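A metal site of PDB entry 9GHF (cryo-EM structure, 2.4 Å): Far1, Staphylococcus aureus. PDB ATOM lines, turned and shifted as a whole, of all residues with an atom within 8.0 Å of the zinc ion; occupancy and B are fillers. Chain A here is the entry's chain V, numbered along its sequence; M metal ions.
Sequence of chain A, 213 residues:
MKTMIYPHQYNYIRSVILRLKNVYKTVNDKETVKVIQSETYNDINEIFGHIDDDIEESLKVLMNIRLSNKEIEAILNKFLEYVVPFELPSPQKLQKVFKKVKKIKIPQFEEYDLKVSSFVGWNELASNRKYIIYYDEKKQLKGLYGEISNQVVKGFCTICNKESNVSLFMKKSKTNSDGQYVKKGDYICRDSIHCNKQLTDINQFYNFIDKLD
The side-chain amide oxygen of Gln 198 sits close to the side-chain sulfur of Cys 189. The side-chain sulfur (SG) of Cys 157 lies close to the backbone NH (N) of Ile 159, 3.3 Å away. O of Lys 162 is in hydrogen-bond range of N of Cys 157 (2.7 Å). The side-chain amide oxygen (OE1) of Gln 198 sits close to the side-chain sulfur (SG) of Cys 160 (3.2 Å). The backbone carbonyl oxygen (O) of Cys 160 is in hydrogen-bond range of the side-chain amino group (NZ) of Lys 162 (2.7 Å). NZ of Lys 162 is in hydrogen-bond range of O of Gln 198, 3.5 Å away. NE2 of Gln 198 lies within hydrogen-bond range of OG of Ser 164, at 2.6 Å. NE2 of Gln 198 lies close to NE2 of His 194, 3.3 Å away.
Merely in contact with the zinc ion: Gln 198. Within 4 Å of the zinc ion: Cys 157, Cys 160, Cys 189, Cys 195 and Gln 198. The nearest printed residue that does not touch the zinc ion is Ile 159 (4.2 Å).
The zinc ion is bound by SG of Cys 195 (2.3 Å), SG of Cys 189 (2.3 Å), SG of Cys 157 (2.3 Å) and SG of Cys 160 (2.3 Å).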
ATOM      1  N   PHE A 119      20.354  15.859 -23.568  1.00  0.00           N
ATOM      2  CA  PHE A 119      19.445  16.363 -24.586  1.00  0.00           C
ATOM      3  C   PHE A 119      20.022  16.060 -25.957  1.00  0.00           C
ATOM      4  O   PHE A 119      21.232  15.873 -26.089  1.00  0.00           O
ATOM      5  CB  PHE A 119      19.252  17.876 -24.419  1.00  0.00           C
ATOM      6  CG  PHE A 119      20.502  18.680 -24.743  1.00  0.00           C
ATOM      7  CD1 PHE A 119      21.452  18.957 -23.760  1.00  0.00           C
ATOM      8  CD2 PHE A 119      20.737  19.156 -26.033  1.00  0.00           C
ATOM      9  CE1 PHE A 119      22.586  19.695 -24.057  1.00  0.00           C
ATOM     10  CE2 PHE A 119      21.871  19.887 -26.318  1.00  0.00           C
ATOM     11  CZ  PHE A 119      22.799  20.154 -25.340  1.00  0.00           C
ATOM     12  N   GLY A 155      34.032  30.820 -26.150  1.00  0.00           N
ATOM     13  CA  GLY A 155      33.435  31.505 -25.011  1.00  0.00           C
ATOM     14  C   GLY A 155      32.736  30.517 -24.085  1.00  0.00           C
ATOM     15  O   GLY A 155      32.435  29.397 -24.483  1.00  0.00           O
ATOM     16  N   PHE A 156      32.484  30.937 -22.838  1.00  0.00           N
ATOM     17  CA  PHE A 156      31.755  30.111 -21.891  1.00  0.00           C
ATOM     18  C   PHE A 156      30.361  29.845 -22.444  1.00  0.00           C
ATOM     19  O   PHE A 156      29.647  30.769 -22.833  1.00  0.00           O
ATOM     20  CB  PHE A 156      31.691  30.743 -20.494  1.00  0.00           C
ATOM     21  CG  PHE A 156      32.800  30.288 -19.550  1.00  0.00           C
ATOM     22  CD1 PHE A 156      34.026  30.946 -19.522  1.00  0.00           C
ATOM     23  CD2 PHE A 156      32.600  29.207 -18.703  1.00  0.00           C
ATOM     24  CE1 PHE A 156      35.030  30.522 -18.665  1.00  0.00           C
ATOM     25  CE2 PHE A 156      33.614  28.784 -17.838  1.00  0.00           C
ATOM     26  CZ  PHE A 156      34.820  29.452 -17.820  1.00  0.00           C
ATOM     27  N   CYS A 157      29.984  28.555 -22.479  1.00  0.00           N
ATOM     28  CA  CYS A 157      28.696  28.131 -23.012  1.00  0.00           C
ATOM     29  C   CYS A 157      27.666  28.100 -21.888  1.00  0.00           C
ATOM     30  O   CYS A 157      27.951  27.572 -20.813  1.00  0.00           O
ATOM     31  CB  CYS A 157      28.809  26.747 -23.649  1.00  0.00           C
ATOM     32  SG  CYS A 157      27.247  25.847 -23.742  1.00  0.00           S
ATOM     33  N   THR A 158      26.478  28.641 -22.152  1.00  0.00           N
ATOM     34  CA  THR A 158      25.458  28.792 -21.129  1.00  0.00           C
ATOM     35  C   THR A 158      24.989  27.417 -20.652  1.00  0.00           C
ATOM     36  O   THR A 158      24.796  27.215 -19.456  1.00  0.00           O
ATOM     37  CB  THR A 158      24.286  29.619 -21.671  1.00  0.00           C
ATOM     38  OG1 THR A 158      24.877  30.790 -22.232  1.00  0.00           O
ATOM     39  CG2 THR A 158      23.297  29.997 -20.587  1.00  0.00           C
ATOM     40  N   ILE A 159      24.819  26.466 -21.584  1.00  0.00           N
ATOM     41  CA  ILE A 159      24.224  25.183 -21.256  1.00  0.00           C
ATOM     42  C   ILE A 159      25.133  24.434 -20.279  1.00  0.00           C
ATOM     43  O   ILE A 159      24.664  23.975 -19.243  1.00  0.00           O
ATOM     44  CB  ILE A 159      23.915  24.347 -22.515  1.00  0.00           C
ATOM     45  CG1 ILE A 159      22.958  25.096 -23.466  1.00  0.00           C
ATOM     46  CG2 ILE A 159      23.366  22.980 -22.133  1.00  0.00           C
ATOM     47  CD1 ILE A 159      22.536  24.309 -24.692  1.00  0.00           C
ATOM     48  N   CYS A 160      26.433  24.318 -20.611  1.00  0.00           N
ATOM     49  CA  CYS A 160      27.351  23.521 -19.799  1.00  0.00           C
ATOM     50  C   CYS A 160      28.113  24.382 -18.804  1.00  0.00           C
ATOM     51  O   CYS A 160      28.735  23.840 -17.888  1.00  0.00           O
ATOM     52  CB  CYS A 160      28.314  22.745 -20.694  1.00  0.00           C
ATOM     53  SG  CYS A 160      29.123  23.750 -21.966  1.00  0.00           S
ATOM     54  N   ASN A 161      28.072  25.717 -18.966  1.00  0.00           N
ATOM     55  CA  ASN A 161      28.798  26.635 -18.102  1.00  0.00           C
ATOM     56  C   ASN A 161      30.306  26.366 -18.200  1.00  0.00           C
ATOM     57  O   ASN A 161      31.018  26.491 -17.208  1.00  0.00           O
ATOM     58  CB  ASN A 161      28.310  26.583 -16.667  1.00  0.00           C
ATOM     59  CG  ASN A 161      26.808  26.709 -16.560  1.00  0.00           C
ATOM     60  OD1 ASN A 161      26.071  25.866 -17.089  1.00  0.00           O
ATOM     61  ND2 ASN A 161      26.328  27.752 -15.890  1.00  0.00           N
ATOM     62  N   LYS A 162      30.770  26.007 -19.412  1.00  0.00           N
ATOM     63  CA  LYS A 162      32.172  25.744 -19.664  1.00  0.00           C
ATOM     64  C   LYS A 162      32.619  26.534 -20.890  1.00  0.00           C
ATOM     65  O   LYS A 162      31.835  26.717 -21.824  1.00  0.00           O
ATOM     66  CB  LYS A 162      32.437  24.258 -19.958  1.00  0.00           C
ATOM     67  CG  LYS A 162      31.809  23.247 -19.015  1.00  0.00           C
ATOM     68  CD  LYS A 162      32.275  23.321 -17.562  1.00  0.00           C
ATOM     69  CE  LYS A 162      31.791  22.168 -16.739  1.00  0.00           C
ATOM     70  NZ  LYS A 162      30.330  22.026 -16.756  1.00  0.00           N
ATOM     71  N   GLU A 163      33.880  26.987 -20.895  1.00  0.00           N
ATOM     72  CA  GLU A 163      34.445  27.681 -22.042  1.00  0.00           C
ATOM     73  C   GLU A 163      34.602  26.665 -23.184  1.00  0.00           C
ATOM     74  O   GLU A 163      35.233  25.630 -23.009  1.00  0.00           O
ATOM     75  CB  GLU A 163      35.765  28.353 -21.678  1.00  0.00           C
ATOM     76  CG  GLU A 163      35.989  29.693 -22.366  1.00  0.00           C
ATOM     77  CD  GLU A 163      36.281  29.667 -23.855  1.00  0.00           C
ATOM     78  OE1 GLU A 163      36.306  28.564 -24.470  1.00  0.00           O
ATOM     79  OE2 GLU A 163      36.491  30.760 -24.408  1.00  0.00           O
ATOM     80  N   SER A 164      34.015  26.997 -24.337  1.00  0.00           N
ATOM     81  CA  SER A 164      34.003  26.115 -25.498  1.00  0.00           C
ATOM     82  C   SER A 164      33.732  26.930 -26.759  1.00  0.00           C
ATOM     83  O   SER A 164      33.413  28.106 -26.681  1.00  0.00           O
ATOM     84  CB  SER A 164      32.978  25.009 -25.332  1.00  0.00           C
ATOM     85  OG  SER A 164      33.259  24.207 -24.198  1.00  0.00           O
ATOM     86  N   ASN A 165      33.866  26.289 -27.935  1.00  0.00           N
ATOM     87  CA  ASN A 165      33.494  26.910 -29.185  1.00  0.00           C
ATOM     88  C   ASN A 165      31.980  27.106 -29.184  1.00  0.00           C
ATOM     89  O   ASN A 165      31.241  26.118 -29.116  1.00  0.00           O
ATOM     90  CB  ASN A 165      33.907  26.090 -30.407  1.00  0.00           C
ATOM     91  CG  ASN A 165      35.373  25.726 -30.398  1.00  0.00           C
ATOM     92  OD1 ASN A 165      36.236  26.611 -30.417  1.00  0.00           O
ATOM     93  ND2 ASN A 165      35.680  24.440 -30.369  1.00  0.00           N
ATOM     94  N   VAL A 166      31.523  28.361 -29.271  1.00  0.00           N
ATOM     95  CA  VAL A 166      30.121  28.673 -29.071  1.00  0.00           C
ATOM     96  C   VAL A 166      29.607  29.551 -30.193  1.00  0.00           C
ATOM     97  O   VAL A 166      30.328  30.400 -30.712  1.00  0.00           O
ATOM     98  CB  VAL A 166      29.876  29.328 -27.689  1.00  0.00           C
ATOM     99  CG1 VAL A 166      30.003  28.323 -26.557  1.00  0.00           C
ATOM    100  CG2 VAL A 166      30.807  30.521 -27.451  1.00  0.00           C
ATOM    101  N   TYR A 187      25.030  32.123 -25.729  1.00  0.00           N
ATOM    102  CA  TYR A 187      25.984  31.334 -26.496  1.00  0.00           C
ATOM    103  C   TYR A 187      25.923  29.889 -25.990  1.00  0.00           C
ATOM    104  O   TYR A 187      25.928  29.650 -24.789  1.00  0.00           O
ATOM    105  CB  TYR A 187      27.401  31.920 -26.393  1.00  0.00           C
ATOM    106  CG  TYR A 187      27.707  33.003 -27.417  1.00  0.00           C
ATOM    107  CD1 TYR A 187      27.464  34.339 -27.145  1.00  0.00           C
ATOM    108  CD2 TYR A 187      28.253  32.682 -28.658  1.00  0.00           C
ATOM    109  CE1 TYR A 187      27.747  35.330 -28.086  1.00  0.00           C
ATOM    110  CE2 TYR A 187      28.533  33.651 -29.604  1.00  0.00           C
ATOM    111  CZ  TYR A 187      28.283  34.991 -29.311  1.00  0.00           C
ATOM    112  OH  TYR A 187      28.565  35.955 -30.235  1.00  0.00           O
ATOM    113  N   ILE A 188      25.862  28.943 -26.947  1.00  0.00           N
ATOM    114  CA  ILE A 188      25.828  27.525 -26.634  1.00  0.00           C
ATOM    115  C   ILE A 188      26.838  26.815 -27.538  1.00  0.00           C
ATOM    116  O   ILE A 188      27.156  27.320 -28.617  1.00  0.00           O
ATOM    117  CB  ILE A 188      24.408  26.968 -26.795  1.00  0.00           C
ATOM    118  CG1 ILE A 188      23.966  26.941 -28.260  1.00  0.00           C
ATOM    119  CG2 ILE A 188      23.423  27.742 -25.917  1.00  0.00           C
ATOM    120  CD1 ILE A 188      22.546  26.450 -28.495  1.00  0.00           C
ATOM    121  N   CYS A 189      27.330  25.658 -27.085  1.00  0.00           N
ATOM    122  CA  CYS A 189      28.328  24.909 -27.845  1.00  0.00           C
ATOM    123  C   CYS A 189      27.769  24.563 -29.220  1.00  0.00           C
ATOM    124  O   CYS A 189      26.612  24.156 -29.339  1.00  0.00           O
ATOM    125  CB  CYS A 189      28.733  23.637 -27.111  1.00  0.00           C
ATOM    126  SG  CYS A 189      29.441  23.915 -25.472  1.00  0.00           S
ATOM    127  N   ARG A 190      28.590  24.734 -30.256  1.00  0.00           N
ATOM    128  CA  ARG A 190      28.178  24.440 -31.617  1.00  0.00           C
ATOM    129  C   ARG A 190      27.883  22.941 -31.730  1.00  0.00           C
ATOM    130  O   ARG A 190      26.911  22.555 -32.380  1.00  0.00           O
ATOM    131  CB  ARG A 190      29.233  24.883 -32.635  1.00  0.00           C
ATOM    132  CG  ARG A 190      28.684  24.957 -34.057  1.00  0.00           C
ATOM    133  CD  ARG A 190      29.730  25.411 -35.076  1.00  0.00           C
ATOM    134  NE  ARG A 190      29.107  25.629 -36.387  1.00  0.00           N
ATOM    135  CZ  ARG A 190      28.256  26.604 -36.688  1.00  0.00           C
ATOM    136  NH1 ARG A 190      28.029  27.594 -35.831  1.00  0.00           N
ATOM    137  NH2 ARG A 190      27.641  26.606 -37.861  1.00  0.00           N
ATOM    138  N   ASP A 191      28.722  22.123 -31.090  1.00  0.00           N
ATOM    139  CA  ASP A 191      28.501  20.689 -31.020  1.00  0.00           C
ATOM    140  C   ASP A 191      27.693  20.358 -29.767  1.00  0.00           C
ATOM    141  O   ASP A 191      28.172  20.552 -28.650  1.00  0.00           O
ATOM    142  CB  ASP A 191      29.820  19.929 -31.045  1.00  0.00           C
ATOM    143  CG  ASP A 191      29.715  18.405 -31.144  1.00  0.00           C
ATOM    144  OD1 ASP A 191      28.570  17.907 -31.256  1.00  0.00           O
ATOM    145  OD2 ASP A 191      30.769  17.739 -31.085  1.00  0.00           O
ATOM    146  N   SER A 192      26.467  19.856 -29.972  1.00  0.00           N
ATOM    147  CA  SER A 192      25.596  19.455 -28.881  1.00  0.00           C
ATOM    148  C   SER A 192      26.179  18.248 -28.150  1.00  0.00           C
ATOM    149  O   SER A 192      26.024  18.117 -26.942  1.00  0.00           O
ATOM    150  CB  SER A 192      24.204  19.160 -29.377  1.00  0.00           C
ATOM    151  OG  SER A 192      23.640  20.289 -30.032  1.00  0.00           O
ATOM    152  N   ILE A 193      26.850  17.364 -28.906  1.00  0.00           N
ATOM    153  CA  ILE A 193      27.406  16.144 -28.344  1.00  0.00           C
ATOM    154  C   ILE A 193      28.537  16.523 -27.383  1.00  0.00           C
ATOM    155  O   ILE A 193      28.601  15.989 -26.280  1.00  0.00           O
ATOM    156  CB  ILE A 193      27.874  15.180 -29.450  1.00  0.00           C
ATOM    157  CG1 ILE A 193      26.791  14.950 -30.510  1.00  0.00           C
ATOM    158  CG2 ILE A 193      28.351  13.853 -28.846  1.00  0.00           C
ATOM    159  CD1 ILE A 193      27.210  14.042 -31.664  1.00  0.00           C
ATOM    160  N   HIS A 194      29.404  17.439 -27.820  1.00  0.00           N
ATOM    161  CA  HIS A 194      30.443  17.980 -26.954  1.00  0.00           C
ATOM    162  C   HIS A 194      29.798  18.606 -25.725  1.00  0.00           C
ATOM    163  O   HIS A 194      30.240  18.364 -24.594  1.00  0.00           O
ATOM    164  CB  HIS A 194      31.295  19.014 -27.702  1.00  0.00           C
ATOM    165  CG  HIS A 194      32.325  19.676 -26.850  1.00  0.00           C
ATOM    166  ND1 HIS A 194      32.705  20.991 -27.026  1.00  0.00           N
ATOM    167  CD2 HIS A 194      33.050  19.224 -25.811  1.00  0.00           C
ATOM    168  CE1 HIS A 194      33.633  21.313 -26.122  1.00  0.00           C
ATOM    169  NE2 HIS A 194      33.858  20.244 -25.378  1.00  0.00           N
ATOM    170  N   CYS A 195      28.742  19.399 -25.954  1.00  0.00           N
ATOM    171  CA  CYS A 195      28.003  20.050 -24.884  1.00  0.00           C
ATOM    172  C   CYS A 195      27.499  19.012 -23.877  1.00  0.00           C
ATOM    173  O   CYS A 195      27.650  19.191 -22.678  1.00  0.00           O
ATOM    174  CB  CYS A 195      26.833  20.829 -25.457  1.00  0.00           C
ATOM    175  SG  CYS A 195      26.100  21.997 -24.280  1.00  0.00           S
ATOM    176  N   ASN A 196      26.897  17.931 -24.403  1.00  0.00           N
ATOM    177  CA  ASN A 196      26.307  16.903 -23.573  1.00  0.00           C
ATOM    178  C   ASN A 196      27.362  16.268 -22.668  1.00  0.00           C
ATOM    179  O   ASN A 196      27.100  16.016 -21.494  1.00  0.00           O
ATOM    180  CB  ASN A 196      25.569  15.858 -24.410  1.00  0.00           C
ATOM    181  CG  ASN A 196      24.171  16.305 -24.763  1.00  0.00           C
ATOM    182  OD1 ASN A 196      23.320  16.454 -23.872  1.00  0.00           O
ATOM    183  ND2 ASN A 196      23.890  16.500 -26.046  1.00  0.00           N
ATOM    184  N   LYS A 197      28.557  16.029 -23.229  1.00  0.00           N
ATOM    185  CA  LYS A 197      29.655  15.450 -22.474  1.00  0.00           C
ATOM    186  C   LYS A 197      30.035  16.379 -21.325  1.00  0.00           C
ATOM    187  O   LYS A 197      30.271  15.926 -20.208  1.00  0.00           O
ATOM    188  CB  LYS A 197      30.880  15.208 -23.357  1.00  0.00           C
ATOM    189  CG  LYS A 197      30.677  14.258 -24.533  1.00  0.00           C
ATOM    190  CD  LYS A 197      31.752  14.380 -25.598  1.00  0.00           C
ATOM    191  CE  LYS A 197      31.468  13.552 -26.811  1.00  0.00           C
ATOM    192  NZ  LYS A 197      32.406  13.824 -27.902  1.00  0.00           N
ATOM    193  N   GLN A 198      30.090  17.687 -21.616  1.00  0.00           N
ATOM    194  CA  GLN A 198      30.491  18.687 -20.649  1.00  0.00           C
ATOM    195  C   GLN A 198      29.467  18.792 -19.514  1.00  0.00           C
ATOM    196  O   GLN A 198      29.847  18.971 -18.361  1.00  0.00           O
ATOM    197  CB  GLN A 198      30.689  20.043 -21.317  1.00  0.00           C
ATOM    198  CG  GLN A 198      31.878  20.096 -22.279  1.00  0.00           C
ATOM    199  CD  GLN A 198      32.044  21.446 -22.942  1.00  0.00           C
ATOM    200  OE1 GLN A 198      31.178  21.915 -23.680  1.00  0.00           O
ATOM    201  NE2 GLN A 198      33.180  22.093 -22.675  1.00  0.00           N
ATOM    202  N   LEU A 199      28.179  18.674 -19.864  1.00  0.00           N
ATOM    203  CA  LEU A 199      27.104  18.829 -18.897  1.00  0.00           C
ATOM    204  C   LEU A 199      27.145  17.692 -17.882  1.00  0.00           C
ATOM    205  O   LEU A 199      27.174  16.525 -18.267  1.00  0.00           O
ATOM    206  CB  LEU A 199      25.768  18.869 -19.625  1.00  0.00           C
ATOM    207  CG  LEU A 199      24.543  19.236 -18.778  1.00  0.00           C
ATOM    208  CD1 LEU A 199      24.635  20.682 -18.291  1.00  0.00           C
ATOM    209  CD2 LEU A 199      23.256  19.026 -19.551  1.00  0.00           C
HETATM  210 ZN    ZN M   1      27.775  23.573 -23.870  1.00  0.00          ZN
